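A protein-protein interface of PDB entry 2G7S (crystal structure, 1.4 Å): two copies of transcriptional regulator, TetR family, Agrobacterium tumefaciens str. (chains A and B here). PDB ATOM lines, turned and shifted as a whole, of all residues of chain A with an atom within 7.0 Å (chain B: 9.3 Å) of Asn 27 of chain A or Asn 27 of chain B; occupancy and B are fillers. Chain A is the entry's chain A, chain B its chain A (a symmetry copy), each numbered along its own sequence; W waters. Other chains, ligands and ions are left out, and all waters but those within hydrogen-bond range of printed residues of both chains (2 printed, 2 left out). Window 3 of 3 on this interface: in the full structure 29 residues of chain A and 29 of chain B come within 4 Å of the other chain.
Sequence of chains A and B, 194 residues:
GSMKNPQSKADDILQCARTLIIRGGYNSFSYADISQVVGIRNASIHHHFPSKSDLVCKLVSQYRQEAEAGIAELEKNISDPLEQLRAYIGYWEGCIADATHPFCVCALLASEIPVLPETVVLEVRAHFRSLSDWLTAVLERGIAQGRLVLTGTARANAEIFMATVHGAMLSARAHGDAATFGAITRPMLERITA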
ATOM      1  N   ILE A  21      -1.316   9.574 -17.039  1.00  0.00           N
ATOM      2  CA  ILE A  21      -1.529   9.149 -18.398  1.00  0.00           C
ATOM      3  C   ILE A  21      -1.515  10.358 -19.370  1.00  0.00           C
ATOM      4  O   ILE A  21      -1.098  10.212 -20.558  1.00  0.00           O
ATOM      5  CB  ILE A  21      -2.793   8.300 -18.506  1.00  0.00           C
ATOM      6  CG1 ILE A  21      -2.666   7.161 -19.456  1.00  0.00           C
ATOM      7  CG2 ILE A  21      -4.034   9.136 -18.473  1.00  0.00           C
ATOM      8  CD1 ILE A  21      -3.783   6.103 -19.361  1.00  0.00           C
ATOM      9  N   GLY A  24       2.168  11.019 -20.593  1.00  0.00           N
ATOM     10  CA  GLY A  24       2.928  10.111 -21.477  1.00  0.00           C
ATOM     11  C   GLY A  24       2.219   8.892 -21.984  1.00  0.00           C
ATOM     12  O   GLY A  24       2.933   8.062 -22.517  1.00  0.00           O
ATOM     13  N   GLY A  25       0.906   8.748 -21.777  1.00  0.00           N
ATOM     14  CA  GLY A  25       0.181   7.612 -22.285  1.00  0.00           C
ATOM     15  C   GLY A  25       0.269   6.357 -21.415  1.00  0.00           C
ATOM     16  O   GLY A  25       0.823   6.328 -20.298  1.00  0.00           O
ATOM     17  N   TYR A  26      -0.245   5.285 -21.982  1.00  0.00           N
ATOM     18  CA  TYR A  26      -0.515   4.064 -21.237  1.00  0.00           C
ATOM     19  C   TYR A  26       0.742   3.493 -20.575  1.00  0.00           C
ATOM     20  O   TYR A  26       0.694   2.944 -19.471  1.00  0.00           O
ATOM     21  CB  TYR A  26      -1.044   3.044 -22.228  1.00  0.00           C
ATOM     22  CG  TYR A  26      -1.559   1.793 -21.552  1.00  0.00           C
ATOM     23  CD1 TYR A  26      -2.844   1.756 -21.011  1.00  0.00           C
ATOM     24  CD2 TYR A  26      -0.769   0.612 -21.493  1.00  0.00           C
ATOM     25  CE1 TYR A  26      -3.333   0.580 -20.386  1.00  0.00           C
ATOM     26  CE2 TYR A  26      -1.286  -0.556 -20.860  1.00  0.00           C
ATOM     27  CZ  TYR A  26      -2.546  -0.536 -20.296  1.00  0.00           C
ATOM     28  OH  TYR A  26      -3.051  -1.639 -19.665  1.00  0.00           O
ATOM     29  N   ASN A  27       1.863   3.535 -21.286  1.00  0.00           N
ATOM     30  CA  ASN A  27       3.096   2.850 -20.863  1.00  0.00           C
ATOM     31  C   ASN A  27       4.055   3.758 -20.140  1.00  0.00           C
ATOM     32  O   ASN A  27       5.216   3.377 -19.883  1.00  0.00           O
ATOM     33  CB  ASN A  27       3.751   2.167 -22.063  1.00  0.00           C
ATOM     34  CG  ASN A  27       3.024   0.905 -22.468  1.00  0.00           C
ATOM     35  OD1 ASN A  27       2.921  -0.011 -21.644  1.00  0.00           O
ATOM     36  ND2 ASN A  27       2.502   0.845 -23.705  1.00  0.00           N
ATOM     37  N   SER A  28       3.618   4.968 -19.831  1.00  0.00           N
ATOM     38  CA  SER A  28       4.528   5.935 -19.210  1.00  0.00           C
ATOM     39  C   SER A  28       4.428   5.928 -17.689  1.00  0.00           C
ATOM     40  O   SER A  28       5.123   6.749 -17.048  1.00  0.00           O
ATOM     41  CB  SER A  28       4.158   7.334 -19.652  1.00  0.00           C
ATOM     42  OG  SER A  28       2.920   7.818 -19.163  1.00  0.00           O
ATOM     43  N   PHE A  29       3.537   5.125 -17.111  1.00  0.00           N
ATOM     44  CA  PHE A  29       3.408   5.043 -15.638  1.00  0.00           C
ATOM     45  C   PHE A  29       3.227   3.610 -15.216  1.00  0.00           C
ATOM     46  O   PHE A  29       2.817   2.766 -16.011  1.00  0.00           O
ATOM     47  CB  PHE A  29       2.272   5.933 -15.125  1.00  0.00           C
ATOM     48  CG  PHE A  29       0.925   5.405 -15.449  1.00  0.00           C
ATOM     49  CD1 PHE A  29       0.243   4.679 -14.478  1.00  0.00           C
ATOM     50  CD2 PHE A  29       0.333   5.521 -16.738  1.00  0.00           C
ATOM     51  CE1 PHE A  29      -1.001   4.103 -14.704  1.00  0.00           C
ATOM     52  CE2 PHE A  29      -0.894   4.909 -16.963  1.00  0.00           C
ATOM     53  CZ  PHE A  29      -1.595   4.229 -15.989  1.00  0.00           C
ATOM     54  N   SER A  30       3.563   3.361 -13.939  1.00  0.00           N
ATOM     55  CA  SER A  30       3.482   2.034 -13.376  1.00  0.00           C
ATOM     56  C   SER A  30       2.651   2.135 -12.081  1.00  0.00           C
ATOM     57  O   SER A  30       2.411   3.235 -11.515  1.00  0.00           O
ATOM     58  CB  SER A  30       4.841   1.524 -12.914  1.00  0.00           C
ATOM     59  OG  SER A  30       5.425   2.438 -12.003  1.00  0.00           O
ATOM     60  N   LYS A  52      -4.094  -3.480 -14.890  1.00  0.00           N
ATOM     61  CA  LYS A  52      -3.889  -2.127 -15.384  1.00  0.00           C
ATOM     62  C   LYS A  52      -4.849  -1.807 -16.522  1.00  0.00           C
ATOM     63  O   LYS A  52      -5.352  -0.653 -16.614  1.00  0.00           O
ATOM     64  CB  LYS A  52      -2.427  -1.983 -15.824  1.00  0.00           C
ATOM     65  CG  LYS A  52      -2.141  -0.587 -16.357  1.00  0.00           C
ATOM     66  CD  LYS A  52      -0.636  -0.539 -16.741  1.00  0.00           C
ATOM     67  CE  LYS A  52      -0.296   0.849 -17.218  1.00  0.00           C
ATOM     68  NZ  LYS A  52       1.202   0.941 -17.576  1.00  0.00           N
ATOM     69  N   LEU A 109      -4.167   8.559 -25.949  1.00  0.00           N
ATOM     70  CA  LEU A 109      -4.176   7.098 -26.073  1.00  0.00           C
ATOM     71  C   LEU A 109      -4.374   6.686 -27.541  1.00  0.00           C
ATOM     72  O   LEU A 109      -3.888   5.629 -27.912  1.00  0.00           O
ATOM     73  CB  LEU A 109      -5.287   6.505 -25.219  1.00  0.00           C
ATOM     74  CG  LEU A 109      -5.004   6.535 -23.706  1.00  0.00           C
ATOM     75  CD1 LEU A 109      -6.270   6.201 -22.909  1.00  0.00           C
ATOM     76  CD2 LEU A 109      -3.878   5.543 -23.283  1.00  0.00           C
ATOM     77  N   GLU A 112      -1.502   5.566 -29.535  1.00  0.00           N
ATOM     78  CA  GLU A 112      -0.813   4.303 -29.128  1.00  0.00           C
ATOM     79  C   GLU A 112      -1.689   3.069 -29.375  1.00  0.00           C
ATOM     80  O   GLU A 112      -1.375   1.968 -28.869  1.00  0.00           O
ATOM     81  CB  GLU A 112      -0.548   4.319 -27.624  1.00  0.00           C
ATOM     82  CG  GLU A 112      -0.021   5.462 -27.070  1.00  0.00           C
ATOM     83  CD  GLU A 112       0.078   5.429 -25.533  1.00  0.00           C
ATOM     84  OE1 GLU A 112      -0.850   5.238 -24.715  1.00  0.00           O
ATOM     85  OE2 GLU A 112       1.103   5.895 -25.178  1.00  0.00           O
ATOM     86  N   VAL A 115      -0.707  -0.809 -29.529  1.00  0.00           N
ATOM     87  CA  VAL A 115      -0.134  -1.531 -28.374  1.00  0.00           C
ATOM     88  C   VAL A 115      -1.087  -1.547 -27.200  1.00  0.00           C
ATOM     89  O   VAL A 115      -0.736  -2.106 -26.144  1.00  0.00           O
ATOM     90  CB  VAL A 115       1.227  -0.978 -27.938  1.00  0.00           C
ATOM     91  CG1 VAL A 115       2.221  -0.991 -29.165  1.00  0.00           C
ATOM     92  CG2 VAL A 115       1.144   0.422 -27.293  1.00  0.00           C
ATOM     93  N   LEU A 116      -2.263  -0.939 -27.327  1.00  0.00           N
ATOM     94  CA  LEU A 116      -3.139  -0.891 -26.145  1.00  0.00           C
ATOM     95  C   LEU A 116      -3.982  -2.175 -26.010  1.00  0.00           C
ATOM     96  O   LEU A 116      -4.331  -2.838 -27.008  1.00  0.00           O
ATOM     97  CB  LEU A 116      -4.155   0.267 -26.274  1.00  0.00           C
ATOM     98  CG  LEU A 116      -3.533   1.652 -26.243  1.00  0.00           C
ATOM     99  CD1 LEU A 116      -4.614   2.720 -26.388  1.00  0.00           C
ATOM    100  CD2 LEU A 116      -2.734   1.902 -24.955  1.00  0.00           C
ATOM    101  N   LEU B  20       8.856  -0.326 -34.018  1.00  0.00           N
ATOM    102  CA  LEU B  20       8.196  -0.484 -32.710  1.00  0.00           C
ATOM    103  C   LEU B  20       7.676   0.865 -32.179  1.00  0.00           C
ATOM    104  O   LEU B  20       6.608   0.936 -31.575  1.00  0.00           O
ATOM    105  CB  LEU B  20       9.126  -1.146 -31.638  1.00  0.00           C
ATOM    106  CG  LEU B  20       9.655  -2.557 -32.077  1.00  0.00           C
ATOM    107  CD1 LEU B  20      10.597  -3.039 -30.994  1.00  0.00           C
ATOM    108  CD2 LEU B  20       8.442  -3.509 -32.256  1.00  0.00           C
ATOM    109  N   ILE B  21       8.480   1.932 -32.342  1.00  0.00           N
ATOM    110  CA  ILE B  21       8.097   3.204 -31.789  1.00  0.00           C
ATOM    111  C   ILE B  21       6.837   3.766 -32.499  1.00  0.00           C
ATOM    112  O   ILE B  21       6.015   4.486 -31.856  1.00  0.00           O
ATOM    113  CB  ILE B  21       9.277   4.173 -31.793  1.00  0.00           C
ATOM    114  CG1 ILE B  21       9.341   5.040 -30.586  1.00  0.00           C
ATOM    115  CG2 ILE B  21       9.532   4.736 -33.156  1.00  0.00           C
ATOM    116  CD1 ILE B  21      10.670   5.796 -30.394  1.00  0.00           C
ATOM    117  N   ILE B  22       6.671   3.444 -33.789  1.00  0.00           N
ATOM    118  CA  ILE B  22       5.473   3.887 -34.491  1.00  0.00           C
ATOM    119  C   ILE B  22       4.209   3.200 -34.005  1.00  0.00           C
ATOM    120  O   ILE B  22       3.077   3.719 -34.180  1.00  0.00           O
ATOM    121  CB  ILE B  22       5.740   3.779 -36.027  1.00  0.00           C
ATOM    122  CG1 ILE B  22       6.760   4.819 -36.432  1.00  0.00           C
ATOM    123  CG2 ILE B  22       4.450   3.990 -36.829  1.00  0.00           C
ATOM    124  CD1 ILE B  22       7.330   4.503 -37.826  1.00  0.00           C
ATOM    125  N   ARG B  23       4.351   2.045 -33.365  1.00  0.00           N
ATOM    126  CA  ARG B  23       3.177   1.400 -32.800  1.00  0.00           C
ATOM    127  C   ARG B  23       2.679   2.017 -31.512  1.00  0.00           C
ATOM    128  O   ARG B  23       1.482   2.022 -31.229  1.00  0.00           O
ATOM    129  CB  ARG B  23       3.421  -0.092 -32.573  1.00  0.00           C
ATOM    130  CG  ARG B  23       3.498  -0.891 -33.894  1.00  0.00           C
ATOM    131  CD  ARG B  23       4.356  -2.109 -33.738  1.00  0.00           C
ATOM    132  NE  ARG B  23       4.183  -2.887 -32.510  1.00  0.00           N
ATOM    133  CZ  ARG B  23       5.042  -2.848 -31.490  1.00  0.00           C
ATOM    134  NH1 ARG B  23       6.046  -2.014 -31.538  1.00  0.00           N
ATOM    135  NH2 ARG B  23       4.898  -3.626 -30.427  1.00  0.00           N
ATOM    136  N   GLY B  24       3.606   2.462 -30.665  1.00  0.00           N
ATOM    137  CA  GLY B  24       3.199   2.868 -29.303  1.00  0.00           C
ATOM    138  C   GLY B  24       4.048   3.888 -28.607  1.00  0.00           C
ATOM    139  O   GLY B  24       3.819   4.029 -27.420  1.00  0.00           O
ATOM    140  N   GLY B  25       5.019   4.519 -29.277  1.00  0.00           N
ATOM    141  CA  GLY B  25       5.829   5.535 -28.655  1.00  0.00           C
ATOM    142  C   GLY B  25       6.999   5.002 -27.827  1.00  0.00           C
ATOM    143  O   GLY B  25       7.313   3.797 -27.772  1.00  0.00           O
ATOM    144  N   TYR B  26       7.613   5.931 -27.124  1.00  0.00           N
ATOM    145  CA  TYR B  26       8.904   5.701 -26.491  1.00  0.00           C
ATOM    146  C   TYR B  26       8.871   4.534 -25.502  1.00  0.00           C
ATOM    147  O   TYR B  26       9.837   3.778 -25.367  1.00  0.00           O
ATOM    148  CB  TYR B  26       9.261   6.967 -25.733  1.00  0.00           C
ATOM    149  CG  TYR B  26      10.674   6.941 -25.196  1.00  0.00           C
ATOM    150  CD1 TYR B  26      11.752   7.273 -26.018  1.00  0.00           C
ATOM    151  CD2 TYR B  26      10.937   6.626 -23.835  1.00  0.00           C
ATOM    152  CE1 TYR B  26      13.078   7.260 -25.513  1.00  0.00           C
ATOM    153  CE2 TYR B  26      12.279   6.622 -23.354  1.00  0.00           C
ATOM    154  CZ  TYR B  26      13.320   6.912 -24.212  1.00  0.00           C
ATOM    155  OH  TYR B  26      14.617   6.891 -23.776  1.00  0.00           O
ATOM    156  N   ASN B  27       7.792   4.432 -24.734  1.00  0.00           N
ATOM    157  CA  ASN B  27       7.706   3.487 -23.609  1.00  0.00           C
ATOM    158  C   ASN B  27       7.013   2.201 -23.972  1.00  0.00           C
ATOM    159  O   ASN B  27       6.699   1.378 -23.086  1.00  0.00           O
ATOM    160  CB  ASN B  27       7.053   4.166 -22.405  1.00  0.00           C
ATOM    161  CG  ASN B  27       7.995   5.123 -21.710  1.00  0.00           C
ATOM    162  OD1 ASN B  27       9.053   4.682 -21.245  1.00  0.00           O
ATOM    163  ND2 ASN B  27       7.647   6.420 -21.648  1.00  0.00           N
ATOM    164  N   SER B  28       6.732   2.012 -25.251  1.00  0.00           N
ATOM    165  CA  SER B  28       5.977   0.825 -25.663  1.00  0.00           C
ATOM    166  C   SER B  28       6.887  -0.321 -26.089  1.00  0.00           C
ATOM    167  O   SER B  28       6.355  -1.372 -26.510  1.00  0.00           O
ATOM    168  CB  SER B  28       5.125   1.160 -26.868  1.00  0.00           C
ATOM    169  OG  SER B  28       5.841   1.419 -28.063  1.00  0.00           O
ATOM    170  N   PHE B  29       8.204  -0.122 -26.093  1.00  0.00           N
ATOM    171  CA  PHE B  29       9.149  -1.200 -26.464  1.00  0.00           C
ATOM    172  C   PHE B  29      10.332  -1.191 -25.535  1.00  0.00           C
ATOM    173  O   PHE B  29      10.625  -0.180 -24.898  1.00  0.00           O
ATOM    174  CB  PHE B  29       9.580  -1.087 -27.929  1.00  0.00           C
ATOM    175  CG  PHE B  29      10.500   0.048 -28.182  1.00  0.00           C
ATOM    176  CD1 PHE B  29      11.867  -0.200 -28.228  1.00  0.00           C
ATOM    177  CD2 PHE B  29      10.060   1.398 -28.286  1.00  0.00           C
ATOM    178  CE1 PHE B  29      12.810   0.805 -28.409  1.00  0.00           C
ATOM    179  CE2 PHE B  29      11.014   2.398 -28.430  1.00  0.00           C
ATOM    180  CZ  PHE B  29      12.367   2.150 -28.522  1.00  0.00           C
ATOM    181  N   SER B  30      10.993  -2.359 -25.465  1.00  0.00           N
ATOM    182  CA  SER B  30      12.134  -2.537 -24.598  1.00  0.00           C
ATOM    183  C   SER B  30      13.285  -3.091 -25.462  1.00  0.00           C
ATOM    184  O   SER B  30      13.095  -3.582 -26.607  1.00  0.00           O
ATOM    185  CB  SER B  30      11.893  -3.616 -23.551  1.00  0.00           C
ATOM    186  OG  SER B  30      11.522  -4.833 -24.175  1.00  0.00           O
ATOM    187  N   TYR B  31      14.467  -3.122 -24.862  1.00  0.00           N
ATOM    188  CA  TYR B  31      15.573  -3.830 -25.546  1.00  0.00           C
ATOM    189  C   TYR B  31      15.249  -5.308 -25.705  1.00  0.00           C
ATOM    190  O   TYR B  31      15.646  -5.899 -26.722  1.00  0.00           O
ATOM    191  CB  TYR B  31      16.893  -3.675 -24.751  1.00  0.00           C
ATOM    192  CG  TYR B  31      17.587  -2.366 -24.967  1.00  0.00           C
ATOM    193  CD1 TYR B  31      16.902  -1.249 -25.518  1.00  0.00           C
ATOM    194  CD2 TYR B  31      18.953  -2.227 -24.695  1.00  0.00           C
ATOM    195  CE1 TYR B  31      17.574  -0.046 -25.706  1.00  0.00           C
ATOM    196  CE2 TYR B  31      19.640  -1.031 -24.906  1.00  0.00           C
ATOM    197  CZ  TYR B  31      18.934   0.058 -25.403  1.00  0.00           C
ATOM    198  OH  TYR B  31      19.601   1.218 -25.630  1.00  0.00           O
ATOM    199  N   ASP B  33      12.457  -6.539 -26.669  1.00  0.00           N
ATOM    200  CA  ASP B  33      11.663  -6.652 -27.877  1.00  0.00           C
ATOM    201  C   ASP B  33      12.602  -6.551 -29.070  1.00  0.00           C
ATOM    202  O   ASP B  33      12.423  -7.275 -30.077  1.00  0.00           O
ATOM    203  CB  ASP B  33      10.671  -5.452 -27.943  1.00  0.00           C
ATOM    204  CG  ASP B  33       9.566  -5.526 -26.899  1.00  0.00           C
ATOM    205  OD1 ASP B  33       9.223  -6.664 -26.430  1.00  0.00           O
ATOM    206  OD2 ASP B  33       9.071  -4.455 -26.519  1.00  0.00           O
ATOM    207  N   LYS B  52      18.973   4.025 -24.079  1.00  0.00           N
ATOM    208  CA  LYS B  52      17.782   4.071 -24.915  1.00  0.00           C
ATOM    209  C   LYS B  52      17.523   5.484 -25.422  1.00  0.00           C
ATOM    210  O   LYS B  52      17.090   5.661 -26.595  1.00  0.00           O
ATOM    211  CB  LYS B  52      16.595   3.539 -24.105  1.00  0.00           C
ATOM    212  CG  LYS B  52      15.310   3.561 -24.919  1.00  0.00           C
ATOM    213  CD  LYS B  52      14.184   2.974 -24.024  1.00  0.00           C
ATOM    214  CE  LYS B  52      12.904   2.922 -24.816  1.00  0.00           C
ATOM    215  NZ  LYS B  52      11.772   2.311 -23.965  1.00  0.00           N
ATOM    216  N   VAL B  56      17.071   6.342 -29.378  1.00  0.00           N
ATOM    217  CA  VAL B  56      15.906   7.051 -29.965  1.00  0.00           C
ATOM    218  C   VAL B  56      16.326   8.413 -30.578  1.00  0.00           C
ATOM    219  O   VAL B  56      15.775   8.786 -31.645  1.00  0.00           O
ATOM    220  CB  VAL B  56      14.812   7.178 -28.901  1.00  0.00           C
ATOM    221  CG1 VAL B  56      13.637   8.030 -29.446  1.00  0.00           C
ATOM    222  CG2 VAL B  56      14.329   5.749 -28.527  1.00  0.00           C
ATOM    223  N   LEU B 108       4.035  11.183 -33.117  1.00  0.00           N
ATOM    224  CA  LEU B 108       3.682  10.287 -32.038  1.00  0.00           C
ATOM    225  C   LEU B 108       4.457  10.684 -30.779  1.00  0.00           C
ATOM    226  O   LEU B 108       3.899  10.771 -29.680  1.00  0.00           O
ATOM    227  CB  LEU B 108       3.919   8.772 -32.463  1.00  0.00           C
ATOM    228  CG  LEU B 108       2.974   7.730 -31.751  1.00  0.00           C
ATOM    229  CD1 LEU B 108       3.060   6.377 -32.447  1.00  0.00           C
ATOM    230  CD2 LEU B 108       3.092   7.576 -30.271  1.00  0.00           C
ATOM    231  N   LEU B 109       5.780  10.833 -30.925  1.00  0.00           N
ATOM    232  CA  LEU B 109       6.574  11.180 -29.741  1.00  0.00           C
ATOM    233  C   LEU B 109       6.114  12.527 -29.162  1.00  0.00           C
ATOM    234  O   LEU B 109       6.242  12.712 -27.962  1.00  0.00           O
ATOM    235  CB  LEU B 109       8.050  11.254 -30.102  1.00  0.00           C
ATOM    236  CG  LEU B 109       8.710   9.884 -30.342  1.00  0.00           C
ATOM    237  CD1 LEU B 109      10.094  10.050 -30.981  1.00  0.00           C
ATOM    238  CD2 LEU B 109       8.869   9.052 -29.033  1.00  0.00           C
ATOM    239  N   GLU B 112       3.974  12.608 -26.180  1.00  0.00           N
ATOM    240  CA  GLU B 112       4.538  12.090 -24.895  1.00  0.00           C
ATOM    241  C   GLU B 112       5.639  13.005 -24.345  1.00  0.00           C
ATOM    242  O   GLU B 112       6.383  12.602 -23.423  1.00  0.00           O
ATOM    243  CB  GLU B 112       5.211  10.739 -25.132  1.00  0.00           C
ATOM    244  CG  GLU B 112       4.540   9.802 -25.881  1.00  0.00           C
ATOM    245  CD  GLU B 112       5.358   8.531 -26.180  1.00  0.00           C
ATOM    246  OE1 GLU B 112       6.472   8.460 -26.749  1.00  0.00           O
ATOM    247  OE2 GLU B 112       4.681   7.570 -26.066  1.00  0.00           O
ATOM    248  N   ILE B 113       5.821  14.192 -24.952  1.00  0.00           N
ATOM    249  CA  ILE B 113       6.938  15.066 -24.536  1.00  0.00           C
ATOM    250  C   ILE B 113       7.219  15.161 -23.039  1.00  0.00           C
ATOM    251  O   ILE B 113       8.380  15.103 -22.629  1.00  0.00           O
ATOM    252  CB  ILE B 113       6.837  16.446 -25.237  1.00  0.00           C
ATOM    253  CG1 ILE B 113       7.419  16.268 -26.678  1.00  0.00           C
ATOM    254  CG2 ILE B 113       7.565  17.528 -24.458  1.00  0.00           C
ATOM    255  CD1 ILE B 113       7.183  17.459 -27.594  1.00  0.00           C
ATOM    256  N   PRO B 114       6.187  15.329 -22.215  1.00  0.00           N
ATOM    257  CA  PRO B 114       6.495  15.549 -20.764  1.00  0.00           C
ATOM    258  C   PRO B 114       7.287  14.396 -20.116  1.00  0.00           C
ATOM    259  O   PRO B 114       7.926  14.628 -19.085  1.00  0.00           O
ATOM    260  CB  PRO B 114       5.092  15.607 -20.108  1.00  0.00           C
ATOM    261  CG  PRO B 114       4.233  16.284 -21.212  1.00  0.00           C
ATOM    262  CD  PRO B 114       4.733  15.546 -22.514  1.00  0.00           C
ATOM    263  N   VAL B 115       7.253  13.193 -20.687  1.00  0.00           N
ATOM    264  CA  VAL B 115       7.985  12.061 -20.081  1.00  0.00           C
ATOM    265  C   VAL B 115       9.208  11.693 -20.890  1.00  0.00           C
ATOM    266  O   VAL B 115       9.919  10.743 -20.512  1.00  0.00           O
ATOM    267  CB  VAL B 115       7.105  10.825 -19.867  1.00  0.00           C
ATOM    268  CG1 VAL B 115       5.845  11.216 -19.000  1.00  0.00           C
ATOM    269  CG2 VAL B 115       6.691  10.130 -21.183  1.00  0.00           C
ATOM    270  N   LEU B 116       9.471  12.383 -21.996  1.00  0.00           N
ATOM    271  CA  LEU B 116      10.616  11.953 -22.815  1.00  0.00           C
ATOM    272  C   LEU B 116      11.940  12.554 -22.301  1.00  0.00           C
ATOM    273  O   LEU B 116      11.976  13.660 -21.723  1.00  0.00           O
ATOM    274  CB  LEU B 116      10.460  12.460 -24.267  1.00  0.00           C
ATOM    275  CG  LEU B 116       9.299  11.840 -25.025  1.00  0.00           C
ATOM    276  CD1 LEU B 116       9.225  12.413 -26.439  1.00  0.00           C
ATOM    277  CD2 LEU B 116       9.402  10.309 -25.096  1.00  0.00           C
ATOM    278  N   PRO B 117      13.044  11.863 -22.578  1.00  0.00           N
ATOM    279  CA  PRO B 117      14.311  12.522 -22.336  1.00  0.00           C
ATOM    280  C   PRO B 117      14.436  13.874 -23.038  1.00  0.00           C
ATOM    281  O   PRO B 117      14.002  13.997 -24.207  1.00  0.00           O
ATOM    282  CB  PRO B 117      15.351  11.519 -22.906  1.00  0.00           C
ATOM    283  CG  PRO B 117      14.637  10.156 -22.979  1.00  0.00           C
ATOM    284  CD  PRO B 117      13.141  10.546 -23.248  1.00  0.00           C
HETATM  285  O   HOH W   1       2.230   3.165 -25.348  1.00  0.00           O
HETATM  286  O   HOH W   2       5.529   7.497 -23.232  1.00  0.00           O
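The side-chain hydroxyl (OG) of Ser 28 of chain A lies close to the backbone carbonyl oxygen (O) of Gly 24 of chain A, 3.4 Å away. The side-chain hydroxyl (OG) of Ser 28 of chain A lies within hydrogen-bond range of the backbone carbonyl oxygen (O) of Gly 25 of chain A. The guanidinium group of Arg 23 of chain B lies close to the backbone carbonyl oxygen of Leu 20 of chain B, at 3.0 Å. The side-chain hydroxyl (OG) of Ser 28 of chain B lies close to the backbone carbonyl oxygen (O) of Gly 24 of chain B. The backbone carbonyl oxygen of Gly 25 of chain B lies within hydrogen-bond range of the side-chain hydroxyl of Ser 28 of chain B, at 2.8 Å. The backbone NH (N) of Tyr 26 of chain B sits at hydrogen-bond distance from the side-chain carboxylate (OE1) of Glu 112 of chain B (2.8 Å).
Glu 112 of chain B touches Gly 24 of chain A. Gly 24 of chain A touches Val 115 of chain B. CB of Asn 27 of chain B touches O of Asn 27 of chain A, at 3.2 Å. Ser 28 of chain B touches Asn 27 of chain A (CA to ND2, 3.99 Å). Asn 27 of chain B touches Ser 28 of chain A (ND2 to CA, 3.99 Å). O of Glu 112 of chain A touches O of Arg 23 of chain B (3.7 Å). Glu 112 of chain A touches Gly 24 of chain B (OE2 to O, 3.99 Å). CB of Arg 23 of chain B touches CG1 of Val 115 of chain A (3.7 Å). Val 115 of chain A touches Gly 24 of chain B.
Printed residues of chain B within 4 Å of Asn 27 of chain A: Asn 27 and Ser 28. Of the printed residues of chain A, Asn 27 of chain B touches Asn 27 and Ser 28. Printed residues of chain A within 4 Å of Gly 24 of chain B: Glu 112 and Val 115. Of the printed residues of chain A, Glu 112 of chain B touches Gly 24 (3.99 Å). The nearest printed residue of chain A that does not touch Asn 27 of chain B is Gly 24 of chain A (5.1 Å). The nearest printed residue of chain A that does not touch Arg 23 of chain B is Leu 116 of chain A (6.2 Å).
Printed residues of chain A that touch a printed residue of chain B: Gly 24, Asn 27, Ser 28, Glu 112 and Val 115. Hydrophobic or aromatic side chains of chain A within 4 Å of the printed part of chain B: Val 115. Along chain A the printed residues that touch a printed residue of chain B span positions 24 to 115. Among the printed residues, no Asp or Glu carboxylate lies within 4 Å of a Lys or Arg side-chain nitrogen of the other chain.
Gly 24 of chain A touches Glu 112 of chain B, and with the chains exchanged Glu 112 of chain A touches Gly 24 of chain B. Gly 24 of chain A touches Val 115 of chain B, and with the chains exchanged Val 115 of chain A touches Gly 24 of chain B. Asn 27 of chain A touches its own counterpart, Asn 27 of chain B. Asn 27 of chain A touches Ser 28 of chain B, and with the chains exchanged Ser 28 of chain A touches Asn 27 of chain B. Of the 9 pairs that touch across the chains among the printed residues, 7 have their exchanged pair printed and touching as well.
Water W1 lies within hydrogen-bond range of the backbone carbonyl oxygen (O) of Gly 24 of chain B (2.8 Å), the side-chain amide nitrogen (ND2) of Asn 27 of chain A (2.9 Å) and the side-chain carboxylate (OE2) of Glu 112 of chain A (3.0 Å). Water W2 lies within hydrogen-bond range of the backbone carbonyl oxygen (O) of Gly 24 of chain A, the side-chain amide nitrogen (ND2) of Asn 27 of chain B and the side-chain carboxylate (OE2) of Glu 112 of chain B.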
